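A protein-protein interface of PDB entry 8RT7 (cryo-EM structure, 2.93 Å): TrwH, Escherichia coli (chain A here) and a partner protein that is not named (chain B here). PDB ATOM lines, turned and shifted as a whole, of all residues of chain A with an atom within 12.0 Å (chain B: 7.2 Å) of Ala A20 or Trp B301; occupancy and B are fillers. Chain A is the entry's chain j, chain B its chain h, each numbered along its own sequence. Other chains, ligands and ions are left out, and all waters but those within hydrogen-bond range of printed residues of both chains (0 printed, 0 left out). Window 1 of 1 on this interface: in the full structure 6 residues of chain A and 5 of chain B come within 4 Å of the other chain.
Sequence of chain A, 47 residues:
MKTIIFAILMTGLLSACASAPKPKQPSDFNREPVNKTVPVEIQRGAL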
ATOM      1  N   CYS A  17      -9.367  -9.540 -20.366  1.00  0.00           N
ATOM      2  CA  CYS A  17      -8.566 -10.687 -20.771  1.00  0.00           C
ATOM      3  C   CYS A  17      -8.364 -11.636 -19.591  1.00  0.00           C
ATOM      4  O   CYS A  17      -8.043 -12.812 -19.772  1.00  0.00           O
ATOM      5  CB  CYS A  17      -7.219 -10.226 -21.329  1.00  0.00           C
ATOM      6  SG  CYS A  17      -6.213 -11.532 -22.065  1.00  0.00           S
ATOM      7  N   ALA A  18      -8.549 -11.114 -18.378  1.00  0.00           N
ATOM      8  CA  ALA A  18      -8.521 -11.920 -17.166  1.00  0.00           C
ATOM      9  C   ALA A  18      -9.563 -11.391 -16.194  1.00  0.00           C
ATOM     10  O   ALA A  18      -9.678 -10.178 -15.996  1.00  0.00           O
ATOM     11  CB  ALA A  18      -7.135 -11.908 -16.511  1.00  0.00           C
ATOM     12  N   SER A  19     -10.315 -12.304 -15.589  1.00  0.00           N
ATOM     13  CA  SER A  19     -11.359 -11.963 -14.637  1.00  0.00           C
ATOM     14  C   SER A  19     -11.001 -12.510 -13.266  1.00  0.00           C
ATOM     15  O   SER A  19     -10.160 -13.400 -13.131  1.00  0.00           O
ATOM     16  CB  SER A  19     -12.721 -12.513 -15.067  1.00  0.00           C
ATOM     17  OG  SER A  19     -13.154 -11.928 -16.278  1.00  0.00           O
ATOM     18  N   ALA A  20     -11.647 -11.960 -12.248  1.00  0.00           N
ATOM     19  CA  ALA A  20     -11.429 -12.429 -10.892  1.00  0.00           C
ATOM     20  C   ALA A  20     -11.929 -13.860 -10.764  1.00  0.00           C
ATOM     21  O   ALA A  20     -13.031 -14.167 -11.225  1.00  0.00           O
ATOM     22  CB  ALA A  20     -12.142 -11.526  -9.901  1.00  0.00           C
ATOM     23  N   PRO A  21     -11.153 -14.761 -10.171  1.00  0.00           N
ATOM     24  CA  PRO A  21     -11.600 -16.150 -10.052  1.00  0.00           C
ATOM     25  C   PRO A  21     -12.843 -16.275  -9.188  1.00  0.00           C
ATOM     26  O   PRO A  21     -13.003 -15.573  -8.191  1.00  0.00           O
ATOM     27  CB  PRO A  21     -10.400 -16.853  -9.416  1.00  0.00           C
ATOM     28  CG  PRO A  21      -9.641 -15.779  -8.758  1.00  0.00           C
ATOM     29  CD  PRO A  21      -9.817 -14.567  -9.601  1.00  0.00           C
ATOM     30  N   LYS A  22     -13.725 -17.175  -9.584  1.00  0.00           N
ATOM     31  CA  LYS A  22     -14.861 -17.525  -8.761  1.00  0.00           C
ATOM     32  C   LYS A  22     -14.408 -18.458  -7.652  1.00  0.00           C
ATOM     33  O   LYS A  22     -13.379 -19.122  -7.775  1.00  0.00           O
ATOM     34  CB  LYS A  22     -15.936 -18.196  -9.604  1.00  0.00           C
ATOM     35  CG  LYS A  22     -16.290 -17.462 -10.879  1.00  0.00           C
ATOM     36  CD  LYS A  22     -16.887 -16.099 -10.588  1.00  0.00           C
ATOM     37  CE  LYS A  22     -18.258 -16.222  -9.960  1.00  0.00           C
ATOM     38  NZ  LYS A  22     -19.029 -17.349 -10.543  1.00  0.00           N
ATOM     39  N   PRO A  23     -15.148 -18.530  -6.550  1.00  0.00           N
ATOM     40  CA  PRO A  23     -14.793 -19.480  -5.499  1.00  0.00           C
ATOM     41  C   PRO A  23     -15.008 -20.905  -5.972  1.00  0.00           C
ATOM     42  O   PRO A  23     -15.619 -21.166  -7.008  1.00  0.00           O
ATOM     43  CB  PRO A  23     -15.736 -19.118  -4.353  1.00  0.00           C
ATOM     44  CG  PRO A  23     -16.231 -17.787  -4.666  1.00  0.00           C
ATOM     45  CD  PRO A  23     -16.272 -17.682  -6.140  1.00  0.00           C
ATOM     46  N   LYS A  24     -14.483 -21.838  -5.188  1.00  0.00           N
ATOM     47  CA  LYS A  24     -14.610 -23.250  -5.506  1.00  0.00           C
ATOM     48  C   LYS A  24     -16.069 -23.641  -5.666  1.00  0.00           C
ATOM     49  O   LYS A  24     -16.921 -23.246  -4.867  1.00  0.00           O
ATOM     50  CB  LYS A  24     -13.971 -24.080  -4.403  1.00  0.00           C
ATOM     51  CG  LYS A  24     -13.949 -25.548  -4.671  1.00  0.00           C
ATOM     52  CD  LYS A  24     -13.227 -26.255  -3.562  1.00  0.00           C
ATOM     53  CE  LYS A  24     -13.187 -27.741  -3.791  1.00  0.00           C
ATOM     54  NZ  LYS A  24     -12.472 -28.412  -2.681  1.00  0.00           N
ATOM     55  N   GLN A  25     -16.356 -24.388  -6.704  1.00  0.00           N
ATOM     56  CA  GLN A  25     -17.676 -24.973  -6.871  1.00  0.00           C
ATOM     57  C   GLN A  25     -17.644 -26.420  -6.424  1.00  0.00           C
ATOM     58  O   GLN A  25     -16.810 -27.191  -6.915  1.00  0.00           O
ATOM     59  CB  GLN A  25     -18.126 -24.891  -8.322  1.00  0.00           C
ATOM     60  CG  GLN A  25     -18.919 -23.652  -8.642  1.00  0.00           C
ATOM     61  CD  GLN A  25     -20.298 -23.673  -8.025  1.00  0.00           C
ATOM     62  OE1 GLN A  25     -20.705 -22.729  -7.349  1.00  0.00           O
ATOM     63  NE2 GLN A  25     -21.029 -24.756  -8.254  1.00  0.00           N
ATOM     64  N   ARG B 220     -17.801 -10.630   0.340  1.00  0.00           N
ATOM     65  CA  ARG B 220     -16.786 -10.550  -0.698  1.00  0.00           C
ATOM     66  C   ARG B 220     -16.202  -9.145  -0.715  1.00  0.00           C
ATOM     67  O   ARG B 220     -16.890  -8.173  -0.412  1.00  0.00           O
ATOM     68  CB  ARG B 220     -17.407 -10.905  -2.040  1.00  0.00           C
ATOM     69  CG  ARG B 220     -16.546 -10.686  -3.232  1.00  0.00           C
ATOM     70  CD  ARG B 220     -17.130 -11.425  -4.400  1.00  0.00           C
ATOM     71  NE  ARG B 220     -16.284 -11.344  -5.579  1.00  0.00           N
ATOM     72  CZ  ARG B 220     -16.596 -10.661  -6.670  1.00  0.00           C
ATOM     73  NH1 ARG B 220     -17.733  -9.996  -6.732  1.00  0.00           N
ATOM     74  NH2 ARG B 220     -15.771 -10.644  -7.700  1.00  0.00           N
ATOM     75  N   LEU B 221     -14.924  -9.028  -1.051  1.00  0.00           N
ATOM     76  CA  LEU B 221     -14.204  -7.775  -0.862  1.00  0.00           C
ATOM     77  C   LEU B 221     -13.623  -7.304  -2.186  1.00  0.00           C
ATOM     78  O   LEU B 221     -12.663  -7.889  -2.688  1.00  0.00           O
ATOM     79  CB  LEU B 221     -13.115  -7.948   0.191  1.00  0.00           C
ATOM     80  CG  LEU B 221     -12.484  -6.711   0.817  1.00  0.00           C
ATOM     81  CD1 LEU B 221     -12.112  -7.029   2.228  1.00  0.00           C
ATOM     82  CD2 LEU B 221     -11.263  -6.322   0.069  1.00  0.00           C
ATOM     83  N   VAL B 222     -14.197  -6.243  -2.741  1.00  0.00           N
ATOM     84  CA  VAL B 222     -13.660  -5.552  -3.905  1.00  0.00           C
ATOM     85  C   VAL B 222     -13.345  -4.132  -3.468  1.00  0.00           C
ATOM     86  O   VAL B 222     -14.222  -3.436  -2.951  1.00  0.00           O
ATOM     87  CB  VAL B 222     -14.645  -5.558  -5.079  1.00  0.00           C
ATOM     88  CG1 VAL B 222     -14.029  -4.888  -6.264  1.00  0.00           C
ATOM     89  CG2 VAL B 222     -15.039  -6.960  -5.417  1.00  0.00           C
ATOM     90  N   LEU B 261      -5.559   0.457  -3.100  1.00  0.00           N
ATOM     91  CA  LEU B 261      -4.187   0.006  -3.243  1.00  0.00           C
ATOM     92  C   LEU B 261      -3.389   0.982  -4.091  1.00  0.00           C
ATOM     93  O   LEU B 261      -3.937   1.760  -4.868  1.00  0.00           O
ATOM     94  CB  LEU B 261      -4.145  -1.383  -3.875  1.00  0.00           C
ATOM     95  CG  LEU B 261      -4.697  -2.500  -3.010  1.00  0.00           C
ATOM     96  CD1 LEU B 261      -4.550  -3.810  -3.705  1.00  0.00           C
ATOM     97  CD2 LEU B 261      -3.961  -2.508  -1.720  1.00  0.00           C
ATOM     98  N   ALA B 266      -0.397  -5.536  -2.887  1.00  0.00           N
ATOM     99  CA  ALA B 266      -1.295  -6.656  -3.103  1.00  0.00           C
ATOM    100  C   ALA B 266      -2.106  -6.999  -1.865  1.00  0.00           C
ATOM    101  O   ALA B 266      -2.708  -8.073  -1.816  1.00  0.00           O
ATOM    102  CB  ALA B 266      -0.508  -7.882  -3.561  1.00  0.00           C
ATOM    103  N   GLY B 299      -5.449  -9.957   1.533  1.00  0.00           N
ATOM    104  CA  GLY B 299      -4.940 -10.091   0.187  1.00  0.00           C
ATOM    105  C   GLY B 299      -5.788 -11.057  -0.607  1.00  0.00           C
ATOM    106  O   GLY B 299      -6.360 -12.000  -0.070  1.00  0.00           O
ATOM    107  N   GLY B 300      -5.860 -10.811  -1.896  1.00  0.00           N
ATOM    108  CA  GLY B 300      -6.655 -11.635  -2.794  1.00  0.00           C
ATOM    109  C   GLY B 300      -6.105 -11.601  -4.180  1.00  0.00           C
ATOM    110  O   GLY B 300      -4.886 -11.675  -4.374  1.00  0.00           O
ATOM    111  N   TRP B 301      -6.989 -11.494  -5.158  1.00  0.00           N
ATOM    112  CA  TRP B 301      -6.611 -11.434  -6.558  1.00  0.00           C
ATOM    113  C   TRP B 301      -6.529  -9.977  -6.982  1.00  0.00           C
ATOM    114  O   TRP B 301      -7.432  -9.195  -6.687  1.00  0.00           O
ATOM    115  CB  TRP B 301      -7.635 -12.194  -7.397  1.00  0.00           C
ATOM    116  CG  TRP B 301      -7.322 -12.268  -8.831  1.00  0.00           C
ATOM    117  CD1 TRP B 301      -6.539 -13.182  -9.445  1.00  0.00           C
ATOM    118  CD2 TRP B 301      -7.794 -11.390  -9.850  1.00  0.00           C
ATOM    119  NE1 TRP B 301      -6.483 -12.928 -10.785  1.00  0.00           N
ATOM    120  CE2 TRP B 301      -7.249 -11.827 -11.057  1.00  0.00           C
ATOM    121  CE3 TRP B 301      -8.626 -10.271  -9.855  1.00  0.00           C
ATOM    122  CZ2 TRP B 301      -7.504 -11.191 -12.255  1.00  0.00           C
ATOM    123  CZ3 TRP B 301      -8.877  -9.643 -11.044  1.00  0.00           C
ATOM    124  CH2 TRP B 301      -8.319 -10.098 -12.226  1.00  0.00           C
ATOM    125  N   ILE B 302      -5.458  -9.608  -7.676  1.00  0.00           N
ATOM    126  CA  ILE B 302      -5.192  -8.214  -8.007  1.00  0.00           C
ATOM    127  C   ILE B 302      -5.415  -8.005  -9.493  1.00  0.00           C
ATOM    128  O   ILE B 302      -4.801  -8.683 -10.322  1.00  0.00           O
ATOM    129  CB  ILE B 302      -3.773  -7.790  -7.611  1.00  0.00           C
ATOM    130  CG1 ILE B 302      -3.525  -8.102  -6.148  1.00  0.00           C
ATOM    131  CG2 ILE B 302      -3.599  -6.321  -7.825  1.00  0.00           C
ATOM    132  CD1 ILE B 302      -4.177  -7.140  -5.233  1.00  0.00           C
ATOM    133  N   ASP B 303      -6.284  -7.061  -9.824  1.00  0.00           N
ATOM    134  CA  ASP B 303      -6.487  -6.617 -11.196  1.00  0.00           C
ATOM    135  C   ASP B 303      -5.606  -5.402 -11.416  1.00  0.00           C
ATOM    136  O   ASP B 303      -5.832  -4.349 -10.819  1.00  0.00           O
ATOM    137  CB  ASP B 303      -7.953  -6.285 -11.438  1.00  0.00           C
ATOM    138  CG  ASP B 303      -8.222  -5.822 -12.841  1.00  0.00           C
ATOM    139  OD1 ASP B 303      -7.379  -6.064 -13.719  1.00  0.00           O
ATOM    140  OD2 ASP B 303      -9.282  -5.216 -13.072  1.00  0.00           O
ATOM    141  N   ARG B 304      -4.591  -5.543 -12.248  1.00  0.00           N
ATOM    142  CA  ARG B 304      -3.652  -4.458 -12.459  1.00  0.00           C
ATOM    143  C   ARG B 304      -4.056  -3.542 -13.597  1.00  0.00           C
ATOM    144  O   ARG B 304      -3.324  -2.596 -13.889  1.00  0.00           O
ATOM    145  CB  ARG B 304      -2.259  -5.018 -12.701  1.00  0.00           C
ATOM    146  CG  ARG B 304      -1.598  -5.463 -11.431  1.00  0.00           C
ATOM    147  CD  ARG B 304      -0.288  -6.142 -11.683  1.00  0.00           C
ATOM    148  NE  ARG B 304       0.135  -6.877 -10.501  1.00  0.00           N
ATOM    149  CZ  ARG B 304      -0.240  -8.120 -10.234  1.00  0.00           C
ATOM    150  NH1 ARG B 304       0.182  -8.719  -9.132  1.00  0.00           N
ATOM    151  NH2 ARG B 304      -1.034  -8.762 -11.074  1.00  0.00           N
ATOM    152  N   THR B 364      -6.788  -3.146  -8.183  1.00  0.00           N
ATOM    153  CA  THR B 364      -8.009  -3.478  -7.465  1.00  0.00           C
ATOM    154  C   THR B 364      -7.902  -4.897  -6.937  1.00  0.00           C
ATOM    155  O   THR B 364      -7.558  -5.812  -7.684  1.00  0.00           O
ATOM    156  CB  THR B 364      -9.232  -3.338  -8.370  1.00  0.00           C
ATOM    157  OG1 THR B 364      -9.342  -1.986  -8.811  1.00  0.00           O
ATOM    158  CG2 THR B 364     -10.486  -3.693  -7.634  1.00  0.00           C
ATOM    159  N   LEU B 365      -8.217  -5.082  -5.665  1.00  0.00           N
ATOM    160  CA  LEU B 365      -8.113  -6.374  -5.012  1.00  0.00           C
ATOM    161  C   LEU B 365      -9.477  -7.034  -4.946  1.00  0.00           C
ATOM    162  O   LEU B 365     -10.477  -6.382  -4.648  1.00  0.00           O
ATOM    163  CB  LEU B 365      -7.539  -6.218  -3.606  1.00  0.00           C
ATOM    164  CG  LEU B 365      -7.171  -7.423  -2.752  1.00  0.00           C
ATOM    165  CD1 LEU B 365      -6.065  -7.011  -1.870  1.00  0.00           C
ATOM    166  CD2 LEU B 365      -8.319  -7.824  -1.896  1.00  0.00           C
ATOM    167  N   TYR B 366      -9.509  -8.330  -5.223  1.00  0.00           N
ATOM    168  CA  TYR B 366     -10.727  -9.127  -5.199  1.00  0.00           C
ATOM    169  C   TYR B 366     -10.513 -10.278  -4.234  1.00  0.00           C
ATOM    170  O   TYR B 366      -9.709 -11.170  -4.504  1.00  0.00           O
ATOM    171  CB  TYR B 366     -11.062  -9.662  -6.586  1.00  0.00           C
ATOM    172  CG  TYR B 366     -11.567  -8.637  -7.553  1.00  0.00           C
ATOM    173  CD1 TYR B 366     -10.712  -7.735  -8.137  1.00  0.00           C
ATOM    174  CD2 TYR B 366     -12.898  -8.587  -7.896  1.00  0.00           C
ATOM    175  CE1 TYR B 366     -11.167  -6.802  -9.009  1.00  0.00           C
ATOM    176  CE2 TYR B 366     -13.360  -7.659  -8.777  1.00  0.00           C
ATOM    177  CZ  TYR B 366     -12.490  -6.765  -9.325  1.00  0.00           C
ATOM    178  OH  TYR B 366     -12.943  -5.827 -10.213  1.00  0.00           O
ATOM    179  N   LYS B 367     -11.243 -10.284  -3.132  1.00  0.00           N
ATOM    180  CA  LYS B 367     -11.160 -11.359  -2.159  1.00  0.00           C
ATOM    181  C   LYS B 367     -12.502 -12.059  -2.089  1.00  0.00           C
ATOM    182  O   LYS B 367     -13.527 -11.416  -1.871  1.00  0.00           O
ATOM    183  CB  LYS B 367     -10.768 -10.823  -0.791  1.00  0.00           C
ATOM    184  CG  LYS B 367     -10.304 -11.873   0.160  1.00  0.00           C
ATOM    185  CD  LYS B 367      -9.739 -11.266   1.399  1.00  0.00           C
ATOM    186  CE  LYS B 367      -9.385 -12.338   2.379  1.00  0.00           C
ATOM    187  NZ  LYS B 367      -8.635 -13.412   1.709  1.00  0.00           N
ATOM    188  N   ASN B 368     -12.495 -13.371  -2.268  1.00  0.00           N
ATOM    189  CA  ASN B 368     -13.739 -14.111  -2.308  1.00  0.00           C
ATOM    190  C   ASN B 368     -14.345 -14.210  -0.918  1.00  0.00           C
ATOM    191  O   ASN B 368     -13.694 -13.969   0.095  1.00  0.00           O
ATOM    192  CB  ASN B 368     -13.512 -15.506  -2.874  1.00  0.00           C
ATOM    193  CG  ASN B 368     -13.434 -15.515  -4.373  1.00  0.00           C
ATOM    194  OD1 ASN B 368     -14.115 -14.750  -5.044  1.00  0.00           O
ATOM    195  ND2 ASN B 368     -12.589 -16.376  -4.910  1.00  0.00           N
ATOM    196  N   GLU B 371     -13.439 -16.846   2.862  1.00  0.00           N
ATOM    197  CA  GLU B 371     -12.030 -17.078   3.115  1.00  0.00           C
ATOM    198  C   GLU B 371     -11.665 -16.767   4.554  1.00  0.00           C
ATOM    199  O   GLU B 371     -12.138 -15.793   5.135  1.00  0.00           O
ATOM    200  CB  GLU B 371     -11.145 -16.264   2.179  1.00  0.00           C
ATOM    201  CG  GLU B 371     -11.231 -16.682   0.738  1.00  0.00           C
ATOM    202  CD  GLU B 371     -10.342 -15.850  -0.146  1.00  0.00           C
ATOM    203  OE1 GLU B 371      -9.758 -14.875   0.358  1.00  0.00           O
ATOM    204  OE2 GLU B 371     -10.207 -16.172  -1.342  1.00  0.00           O
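Hydrophobic or aromatic side chains of chain A that line the printed part of chain B: Ala A20, Pro A21 and Pro A23. Of the 17 printed residues of chain B, 3 touch a printed residue of chain A. Hydrophobic or aromatic side chains of chain B within 4 Å of the printed part of chain A: Trp B301 and Tyr B366. Among the printed residues, 7 pairs touch across the chains. Among the printed residues, no Asp or Glu carboxylate lies within 4 Å of a Lys or Arg side-chain nitrogen of the other chain.
O of Trp B301 lies within hydrogen-bond range of N of Tyr B366 (2.7 Å).
Printed residues of chain B within 4 Å of Ser A19: Trp B301. Ala A20 touches just these residues of chain B: Trp B301 (3.7 Å) and Tyr B366 (3.6 Å). Printed residues of chain B within 4 Å of Pro A23: Asn B368 (3.6 Å). No residue of chain A comes within 4 Å of Gly B300. Of the printed residues of chain A, Trp B301 touches Ser A19, Ala A20 and Pro A21. Ile B302 touches none of the printed residues of chain A. No residue of chain A comes within 4 Å of Asp B303. Tyr B366 touches one residue of chain A.
Trp B301 touches Ser A19 (CZ2 to O, 3.6 Å). CA of Ala A20 touches CE3 of Trp B301, at 3.7 Å. Ala A20 touches Tyr B366. Pro A21 touches Trp B301 (CD to CG, 3.5 Å). Lys A22 touches Asn B368 (C to ND2, 3.9 Å). Pro A23 touches Asn B368 (CG to CG, 3.6 Å).
The backbone carbonyl oxygen (O) of Pro A21 lies within hydrogen-bond range of the side-chain amide nitrogen (ND2) of Asn B368, 3.4 Å away.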
